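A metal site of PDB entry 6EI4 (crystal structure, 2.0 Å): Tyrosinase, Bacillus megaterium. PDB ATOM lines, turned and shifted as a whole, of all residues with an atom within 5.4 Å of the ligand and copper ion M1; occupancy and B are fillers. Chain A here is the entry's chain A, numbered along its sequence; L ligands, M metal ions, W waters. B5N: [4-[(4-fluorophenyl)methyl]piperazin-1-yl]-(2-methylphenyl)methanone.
The guanidinium group (NH1) of Arg 206 is in hydrogen-bond range of an oxygen (O22) of the ligand (3.1 Å).
A ring nitrogen (ND1) of His 205 is in hydrogen-bond range of the backbone carbonyl oxygen (O) of Met 212 (3.0 Å). O of Gly 193 lies within hydrogen-bond range of N of Gln 199, 3.2 Å away. ND1 of His 66 lies within hydrogen-bond range of O of Phe 62 (2.7 Å). The side-chain amide oxygen (OD1) of Asn 202 sits at hydrogen-bond distance from a ring nitrogen (ND1) of His 201 (2.9 Å). The side-chain amide nitrogen (ND2) of Asn 202 lies within hydrogen-bond range of the backbone carbonyl oxygen (O) of Gly 193 (3.4 Å). The backbone carbonyl oxygen (O) of Val 215 sits close to a ring nitrogen (ND1) of His 39 (2.9 Å).
Residues that only touch the ligand: Gly 193, Phe 194, Pro 198, His 201, Asn 202, His 205, Gly 213, Val 214, Val 215, Ala 218, Phe 224 and His 228. Hydrophobic or aromatic side chains within 4 Å of the ligand: His 39, His 57, Phe 194, Pro 198, His 201, His 205, Val 215, Ala 218 and Phe 224. Of the 22 residues printed, 16 come within 4 Å of the ligand. The nearest printed residue that does not touch the ligand is Met 212 (4.01 Å).
CZ of Phe 224 touches copper ion M1 (3.96 Å). Four residues have an atom within 4 Å of copper ion M1: His 39, His 57, His 66 and Phe 224. The nearest printed residue that does not touch copper ion M1 is His 228 (4.05 Å).
Copper ion M1 is bound by NE2 of His 57, F07 of the ligand, NE2 of His 39 and NE2 of His 66. Copper ion M1 has four donor atoms within binding distance.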
ATOM      1  N   HIS A  39     -20.976  35.247  -1.237  1.00  0.00           N
ATOM      2  CA  HIS A  39     -20.237  34.127  -1.805  1.00  0.00           C
ATOM      3  C   HIS A  39     -21.177  33.020  -2.252  1.00  0.00           C
ATOM      4  O   HIS A  39     -21.022  32.461  -3.341  1.00  0.00           O
ATOM      5  CB  HIS A  39     -19.228  33.594  -0.781  1.00  0.00           C
ATOM      6  CG  HIS A  39     -18.286  32.579  -1.327  1.00  0.00           C
ATOM      7  ND1 HIS A  39     -18.387  31.230  -1.054  1.00  0.00           N
ATOM      8  CD2 HIS A  39     -17.213  32.714  -2.144  1.00  0.00           C
ATOM      9  CE1 HIS A  39     -17.417  30.586  -1.671  1.00  0.00           C
ATOM     10  NE2 HIS A  39     -16.691  31.461  -2.344  1.00  0.00           N
ATOM     11  N   ALA A  56     -18.408  33.469  -9.344  1.00  0.00           N
ATOM     12  CA  ALA A  56     -17.216  33.485  -8.499  1.00  0.00           C
ATOM     13  C   ALA A  56     -16.267  32.296  -8.713  1.00  0.00           C
ATOM     14  O   ALA A  56     -15.136  32.338  -8.249  1.00  0.00           O
ATOM     15  CB  ALA A  56     -17.628  33.551  -7.046  1.00  0.00           C
ATOM     16  N   HIS A  57     -16.722  31.253  -9.407  1.00  0.00           N
ATOM     17  CA  HIS A  57     -15.901  30.046  -9.534  1.00  0.00           C
ATOM     18  C   HIS A  57     -16.047  29.360 -10.877  1.00  0.00           C
ATOM     19  O   HIS A  57     -16.977  29.633 -11.642  1.00  0.00           O
ATOM     20  CB  HIS A  57     -16.259  29.035  -8.441  1.00  0.00           C
ATOM     21  CG  HIS A  57     -16.296  29.618  -7.057  1.00  0.00           C
ATOM     22  ND1 HIS A  57     -17.438  30.139  -6.508  1.00  0.00           N
ATOM     23  CD2 HIS A  57     -15.329  29.742  -6.122  1.00  0.00           C
ATOM     24  CE1 HIS A  57     -17.178  30.573  -5.289  1.00  0.00           C
ATOM     25  NE2 HIS A  57     -15.904  30.343  -5.031  1.00  0.00           N
ATOM     26  N   PHE A  62     -13.055  34.061 -11.450  1.00  0.00           N
ATOM     27  CA  PHE A  62     -12.705  33.495 -10.151  1.00  0.00           C
ATOM     28  C   PHE A  62     -11.709  34.347  -9.375  1.00  0.00           C
ATOM     29  O   PHE A  62     -11.919  34.637  -8.190  1.00  0.00           O
ATOM     30  CB  PHE A  62     -12.142  32.085 -10.327  1.00  0.00           C
ATOM     31  CG  PHE A  62     -11.445  31.549  -9.100  1.00  0.00           C
ATOM     32  CD1 PHE A  62     -12.167  31.201  -7.968  1.00  0.00           C
ATOM     33  CD2 PHE A  62     -10.062  31.386  -9.081  1.00  0.00           C
ATOM     34  CE1 PHE A  62     -11.525  30.712  -6.840  1.00  0.00           C
ATOM     35  CE2 PHE A  62      -9.424  30.904  -7.965  1.00  0.00           C
ATOM     36  CZ  PHE A  62     -10.154  30.556  -6.838  1.00  0.00           C
ATOM     37  N   TRP A  65     -12.980  38.184  -8.818  1.00  0.00           N
ATOM     38  CA  TRP A  65     -14.151  38.199  -7.942  1.00  0.00           C
ATOM     39  C   TRP A  65     -13.731  38.120  -6.484  1.00  0.00           C
ATOM     40  O   TRP A  65     -14.251  38.847  -5.639  1.00  0.00           O
ATOM     41  CB  TRP A  65     -15.094  37.034  -8.276  1.00  0.00           C
ATOM     42  CG  TRP A  65     -16.411  37.097  -7.558  1.00  0.00           C
ATOM     43  CD1 TRP A  65     -17.603  37.522  -8.084  1.00  0.00           C
ATOM     44  CD2 TRP A  65     -16.684  36.712  -6.198  1.00  0.00           C
ATOM     45  NE1 TRP A  65     -18.588  37.433  -7.128  1.00  0.00           N
ATOM     46  CE2 TRP A  65     -18.056  36.943  -5.979  1.00  0.00           C
ATOM     47  CE3 TRP A  65     -15.900  36.198  -5.161  1.00  0.00           C
ATOM     48  CZ2 TRP A  65     -18.655  36.680  -4.740  1.00  0.00           C
ATOM     49  CZ3 TRP A  65     -16.498  35.948  -3.940  1.00  0.00           C
ATOM     50  CH2 TRP A  65     -17.866  36.185  -3.744  1.00  0.00           C
ATOM     51  N   HIS A  66     -12.778  37.233  -6.187  1.00  0.00           N
ATOM     52  CA  HIS A  66     -12.336  37.070  -4.818  1.00  0.00           C
ATOM     53  C   HIS A  66     -11.420  38.205  -4.389  1.00  0.00           C
ATOM     54  O   HIS A  66     -11.359  38.525  -3.216  1.00  0.00           O
ATOM     55  CB  HIS A  66     -11.642  35.716  -4.627  1.00  0.00           C
ATOM     56  CG  HIS A  66     -12.591  34.553  -4.660  1.00  0.00           C
ATOM     57  ND1 HIS A  66     -13.017  33.980  -5.848  1.00  0.00           N
ATOM     58  CD2 HIS A  66     -13.207  33.874  -3.678  1.00  0.00           C
ATOM     59  CE1 HIS A  66     -13.836  32.990  -5.582  1.00  0.00           C
ATOM     60  NE2 HIS A  66     -13.970  32.901  -4.265  1.00  0.00           N
ATOM     61  N   GLY A 193      -7.652  25.199  -9.378  1.00  0.00           N
ATOM     62  CA  GLY A 193      -7.331  23.836  -8.981  1.00  0.00           C
ATOM     63  C   GLY A 193      -8.096  22.743  -9.696  1.00  0.00           C
ATOM     64  O   GLY A 193      -8.360  21.687  -9.113  1.00  0.00           O
ATOM     65  N   PHE A 194      -8.409  22.962 -10.968  1.00  0.00           N
ATOM     66  CA  PHE A 194      -9.210  21.996 -11.717  1.00  0.00           C
ATOM     67  C   PHE A 194      -8.380  21.163 -12.690  1.00  0.00           C
ATOM     68  O   PHE A 194      -8.896  20.261 -13.326  1.00  0.00           O
ATOM     69  CB  PHE A 194     -10.339  22.705 -12.462  1.00  0.00           C
ATOM     70  CG  PHE A 194     -11.514  23.052 -11.590  1.00  0.00           C
ATOM     71  CD1 PHE A 194     -12.295  22.054 -11.036  1.00  0.00           C
ATOM     72  CD2 PHE A 194     -11.842  24.372 -11.319  1.00  0.00           C
ATOM     73  CE1 PHE A 194     -13.377  22.351 -10.235  1.00  0.00           C
ATOM     74  CE2 PHE A 194     -12.923  24.683 -10.519  1.00  0.00           C
ATOM     75  CZ  PHE A 194     -13.689  23.669  -9.971  1.00  0.00           C
ATOM     76  N   GLY A 197      -7.605  17.945 -10.760  1.00  0.00           N
ATOM     77  CA  GLY A 197      -8.024  18.380  -9.435  1.00  0.00           C
ATOM     78  C   GLY A 197      -8.391  17.263  -8.475  1.00  0.00           C
ATOM     79  O   GLY A 197      -8.608  16.131  -8.896  1.00  0.00           O
ATOM     80  N   PRO A 198      -8.460  17.588  -7.175  1.00  0.00           N
ATOM     81  CA  PRO A 198      -8.245  18.926  -6.619  1.00  0.00           C
ATOM     82  C   PRO A 198      -6.776  19.287  -6.392  1.00  0.00           C
ATOM     83  O   PRO A 198      -6.017  18.501  -5.832  1.00  0.00           O
ATOM     84  CB  PRO A 198      -8.982  18.866  -5.276  1.00  0.00           C
ATOM     85  CG  PRO A 198      -8.898  17.436  -4.883  1.00  0.00           C
ATOM     86  CD  PRO A 198      -9.001  16.659  -6.166  1.00  0.00           C
ATOM     87  N   GLN A 199      -6.398  20.495  -6.819  1.00  0.00           N
ATOM     88  CA  GLN A 199      -5.060  21.018  -6.607  1.00  0.00           C
ATOM     89  C   GLN A 199      -5.129  22.464  -6.127  1.00  0.00           C
ATOM     90  O   GLN A 199      -6.154  23.119  -6.300  1.00  0.00           O
ATOM     91  CB  GLN A 199      -4.218  20.928  -7.878  1.00  0.00           C
ATOM     92  CG  GLN A 199      -4.018  19.517  -8.393  1.00  0.00           C
ATOM     93  CD  GLN A 199      -3.231  18.665  -7.420  1.00  0.00           C
ATOM     94  OE1 GLN A 199      -2.502  19.179  -6.571  1.00  0.00           O
ATOM     95  NE2 GLN A 199      -3.380  17.348  -7.528  1.00  0.00           N
ATOM     96  N   HIS A 201      -5.782  25.923  -4.788  1.00  0.00           N
ATOM     97  CA  HIS A 201      -6.931  26.521  -4.115  1.00  0.00           C
ATOM     98  C   HIS A 201      -8.018  25.507  -3.734  1.00  0.00           C
ATOM     99  O   HIS A 201      -8.422  25.430  -2.569  1.00  0.00           O
ATOM    100  CB  HIS A 201      -7.559  27.619  -4.979  1.00  0.00           C
ATOM    101  CG  HIS A 201      -8.951  27.987  -4.580  1.00  0.00           C
ATOM    102  ND1 HIS A 201     -10.070  27.428  -5.164  1.00  0.00           N
ATOM    103  CD2 HIS A 201      -9.416  28.851  -3.651  1.00  0.00           C
ATOM    104  CE1 HIS A 201     -11.155  27.932  -4.610  1.00  0.00           C
ATOM    105  NE2 HIS A 201     -10.790  28.806  -3.690  1.00  0.00           N
ATOM    106  N   ASN A 202      -8.506  24.756  -4.719  1.00  0.00           N
ATOM    107  CA  ASN A 202      -9.535  23.754  -4.463  1.00  0.00           C
ATOM    108  C   ASN A 202      -9.076  22.706  -3.468  1.00  0.00           C
ATOM    109  O   ASN A 202      -9.872  22.233  -2.645  1.00  0.00           O
ATOM    110  CB  ASN A 202      -9.945  23.074  -5.767  1.00  0.00           C
ATOM    111  CG  ASN A 202     -10.813  23.955  -6.652  1.00  0.00           C
ATOM    112  OD1 ASN A 202     -11.321  24.980  -6.204  1.00  0.00           O
ATOM    113  ND2 ASN A 202     -10.995  23.552  -7.897  1.00  0.00           N
ATOM    114  N   HIS A 205      -9.301  24.011   0.317  1.00  0.00           N
ATOM    115  CA  HIS A 205     -10.668  23.879   0.797  1.00  0.00           C
ATOM    116  C   HIS A 205     -10.984  22.442   1.234  1.00  0.00           C
ATOM    117  O   HIS A 205     -11.463  22.210   2.345  1.00  0.00           O
ATOM    118  CB  HIS A 205     -11.662  24.331  -0.269  1.00  0.00           C
ATOM    119  CG  HIS A 205     -11.806  25.821  -0.367  1.00  0.00           C
ATOM    120  ND1 HIS A 205     -12.347  26.579   0.639  1.00  0.00           N
ATOM    121  CD2 HIS A 205     -11.460  26.683  -1.355  1.00  0.00           C
ATOM    122  CE1 HIS A 205     -12.327  27.857   0.286  1.00  0.00           C
ATOM    123  NE2 HIS A 205     -11.805  27.947  -0.930  1.00  0.00           N
ATOM    124  N   ARG A 206     -10.693  21.490   0.350  1.00  0.00           N
ATOM    125  CA  ARG A 206     -10.931  20.084   0.632  1.00  0.00           C
ATOM    126  C   ARG A 206     -10.110  19.611   1.834  1.00  0.00           C
ATOM    127  O   ARG A 206     -10.606  18.870   2.688  1.00  0.00           O
ATOM    128  CB  ARG A 206     -10.607  19.226  -0.593  1.00  0.00           C
ATOM    129  CG  ARG A 206     -11.363  19.629  -1.840  1.00  0.00           C
ATOM    130  CD  ARG A 206     -12.781  19.071  -1.839  1.00  0.00           C
ATOM    131  NE  ARG A 206     -12.809  17.651  -1.496  1.00  0.00           N
ATOM    132  CZ  ARG A 206     -12.716  16.665  -2.387  1.00  0.00           C
ATOM    133  NH1 ARG A 206     -12.592  16.948  -3.667  1.00  0.00           N
ATOM    134  NH2 ARG A 206     -12.750  15.405  -1.976  1.00  0.00           N
ATOM    135  N   MET A 212     -15.423  24.786   5.160  1.00  0.00           N
ATOM    136  CA  MET A 212     -14.473  25.149   4.117  1.00  0.00           C
ATOM    137  C   MET A 212     -14.513  24.155   2.953  1.00  0.00           C
ATOM    138  O   MET A 212     -14.083  24.468   1.846  1.00  0.00           O
ATOM    139  CB  MET A 212     -13.047  25.232   4.678  1.00  0.00           C
ATOM    140  CG  MET A 212     -12.695  26.585   5.263  1.00  0.00           C
ATOM    141  SD  MET A 212     -12.365  27.830   3.996  1.00  0.00           S
ATOM    142  CE  MET A 212     -10.683  27.416   3.537  1.00  0.00           C
ATOM    143  N   GLY A 213     -15.040  22.967   3.223  1.00  0.00           N
ATOM    144  CA  GLY A 213     -15.097  21.905   2.231  1.00  0.00           C
ATOM    145  C   GLY A 213     -16.224  22.018   1.215  1.00  0.00           C
ATOM    146  O   GLY A 213     -16.245  21.260   0.248  1.00  0.00           O
ATOM    147  N   VAL A 214     -17.174  22.918   1.444  1.00  0.00           N
ATOM    148  CA  VAL A 214     -18.233  23.150   0.454  1.00  0.00           C
ATOM    149  C   VAL A 214     -18.339  24.649   0.152  1.00  0.00           C
ATOM    150  O   VAL A 214     -18.181  25.488   1.041  1.00  0.00           O
ATOM    151  CB  VAL A 214     -19.610  22.585   0.904  1.00  0.00           C
ATOM    152  CG1 VAL A 214     -19.450  21.206   1.528  1.00  0.00           C
ATOM    153  CG2 VAL A 214     -20.316  23.518   1.874  1.00  0.00           C
ATOM    154  N   VAL A 215     -18.566  24.934  -1.121  1.00  0.00           N
ATOM    155  CA  VAL A 215     -18.647  26.292  -1.665  1.00  0.00           C
ATOM    156  C   VAL A 215     -19.564  27.305  -0.993  1.00  0.00           C
ATOM    157  O   VAL A 215     -19.145  28.439  -0.753  1.00  0.00           O
ATOM    158  CB  VAL A 215     -18.988  26.258  -3.172  1.00  0.00           C
ATOM    159  CG1 VAL A 215     -18.588  27.566  -3.831  1.00  0.00           C
ATOM    160  CG2 VAL A 215     -18.304  25.079  -3.839  1.00  0.00           C
ATOM    161  N   ALA A 218     -18.221  27.907   2.958  1.00  0.00           N
ATOM    162  CA  ALA A 218     -16.787  28.082   3.254  1.00  0.00           C
ATOM    163  C   ALA A 218     -16.432  29.374   4.015  1.00  0.00           C
ATOM    164  O   ALA A 218     -15.605  29.319   4.941  1.00  0.00           O
ATOM    165  CB  ALA A 218     -15.990  28.014   1.961  1.00  0.00           C
ATOM    166  N   PHE A 224     -10.892  31.298   5.631  1.00  0.00           N
ATOM    167  CA  PHE A 224     -11.248  31.398   4.222  1.00  0.00           C
ATOM    168  C   PHE A 224     -10.600  32.634   3.621  1.00  0.00           C
ATOM    169  O   PHE A 224     -10.118  32.609   2.482  1.00  0.00           O
ATOM    170  CB  PHE A 224     -12.776  31.453   4.057  1.00  0.00           C
ATOM    171  CG  PHE A 224     -13.259  31.801   2.664  1.00  0.00           C
ATOM    172  CD1 PHE A 224     -13.317  33.113   2.230  1.00  0.00           C
ATOM    173  CD2 PHE A 224     -13.669  30.804   1.792  1.00  0.00           C
ATOM    174  CE1 PHE A 224     -13.772  33.423   0.959  1.00  0.00           C
ATOM    175  CE2 PHE A 224     -14.112  31.106   0.521  1.00  0.00           C
ATOM    176  CZ  PHE A 224     -14.170  32.420   0.105  1.00  0.00           C
ATOM    177  N   HIS A 228      -7.684  32.868   0.757  1.00  0.00           N
ATOM    178  CA  HIS A 228      -7.823  33.553  -0.515  1.00  0.00           C
ATOM    179  C   HIS A 228      -6.859  34.727  -0.651  1.00  0.00           C
ATOM    180  O   HIS A 228      -6.519  35.122  -1.765  1.00  0.00           O
ATOM    181  CB  HIS A 228      -9.272  34.007  -0.720  1.00  0.00           C
ATOM    182  CG  HIS A 228     -10.126  32.971  -1.371  1.00  0.00           C
ATOM    183  ND1 HIS A 228     -10.144  32.759  -2.737  1.00  0.00           N
ATOM    184  CD2 HIS A 228     -10.966  32.052  -0.837  1.00  0.00           C
ATOM    185  CE1 HIS A 228     -10.970  31.763  -3.009  1.00  0.00           C
ATOM    186  NE2 HIS A 228     -11.484  31.320  -1.886  1.00  0.00           N
HETATM  187  C01 B5N L   1     -14.487  26.323  -3.768  1.00  0.00           C
HETATM  188  C02 B5N L   1     -14.324  27.714  -3.716  1.00  0.00           C
HETATM  189  C03 B5N L   1     -15.062  25.640  -2.682  1.00  0.00           C
HETATM  190  C04 B5N L   1     -14.733  28.415  -2.602  1.00  0.00           C
HETATM  191  C05 B5N L   1     -15.459  26.347  -1.569  1.00  0.00           C
HETATM  192  C06 B5N L   1     -15.304  27.739  -1.522  1.00  0.00           C
HETATM  193  C08 B5N L   1     -15.240  24.108  -2.732  1.00  0.00           C
HETATM  194  C10 B5N L   1     -14.917  21.285  -2.476  1.00  0.00           C
HETATM  195  C11 B5N L   1     -14.361  22.418  -1.588  1.00  0.00           C
HETATM  196  C13 B5N L   1     -13.506  22.465  -4.301  1.00  0.00           C
HETATM  197  C14 B5N L   1     -13.164  23.430  -3.141  1.00  0.00           C
HETATM  198  C15 B5N L   1     -14.240  20.004  -4.578  1.00  0.00           C
HETATM  199  C16 B5N L   1     -13.501  19.962  -5.964  1.00  0.00           C
HETATM  200  C17 B5N L   1     -13.544  19.445  -8.320  1.00  0.00           C
HETATM  201  C18 B5N L   1     -14.182  19.488  -7.106  1.00  0.00           C
HETATM  202  C19 B5N L   1     -12.189  19.880  -8.427  1.00  0.00           C
HETATM  203  C20 B5N L   1     -11.522  20.347  -7.301  1.00  0.00           C
HETATM  204  C21 B5N L   1     -12.172  20.384  -6.070  1.00  0.00           C
HETATM  205  C23 B5N L   1     -15.631  19.023  -6.982  1.00  0.00           C
HETATM  206  F07 B5N L   1     -14.575  29.786  -2.543  1.00  0.00           F
HETATM  207  N09 B5N L   1     -14.123  23.513  -2.259  1.00  0.00           N
HETATM  208  N12 B5N L   1     -14.224  21.264  -3.774  1.00  0.00           N
HETATM  209  O22 B5N L   1     -14.812  19.031  -4.161  1.00  0.00           O
HETATM  210 CU    CU M   1     -15.172  31.285  -3.555  1.00  0.00          CU
HETATM  211 CU    CU M   2     -12.003  29.431  -2.298  1.00  0.00          CU
HETATM  212  O   HOH W   1     -15.834  25.899  -6.611  1.00  0.00           O
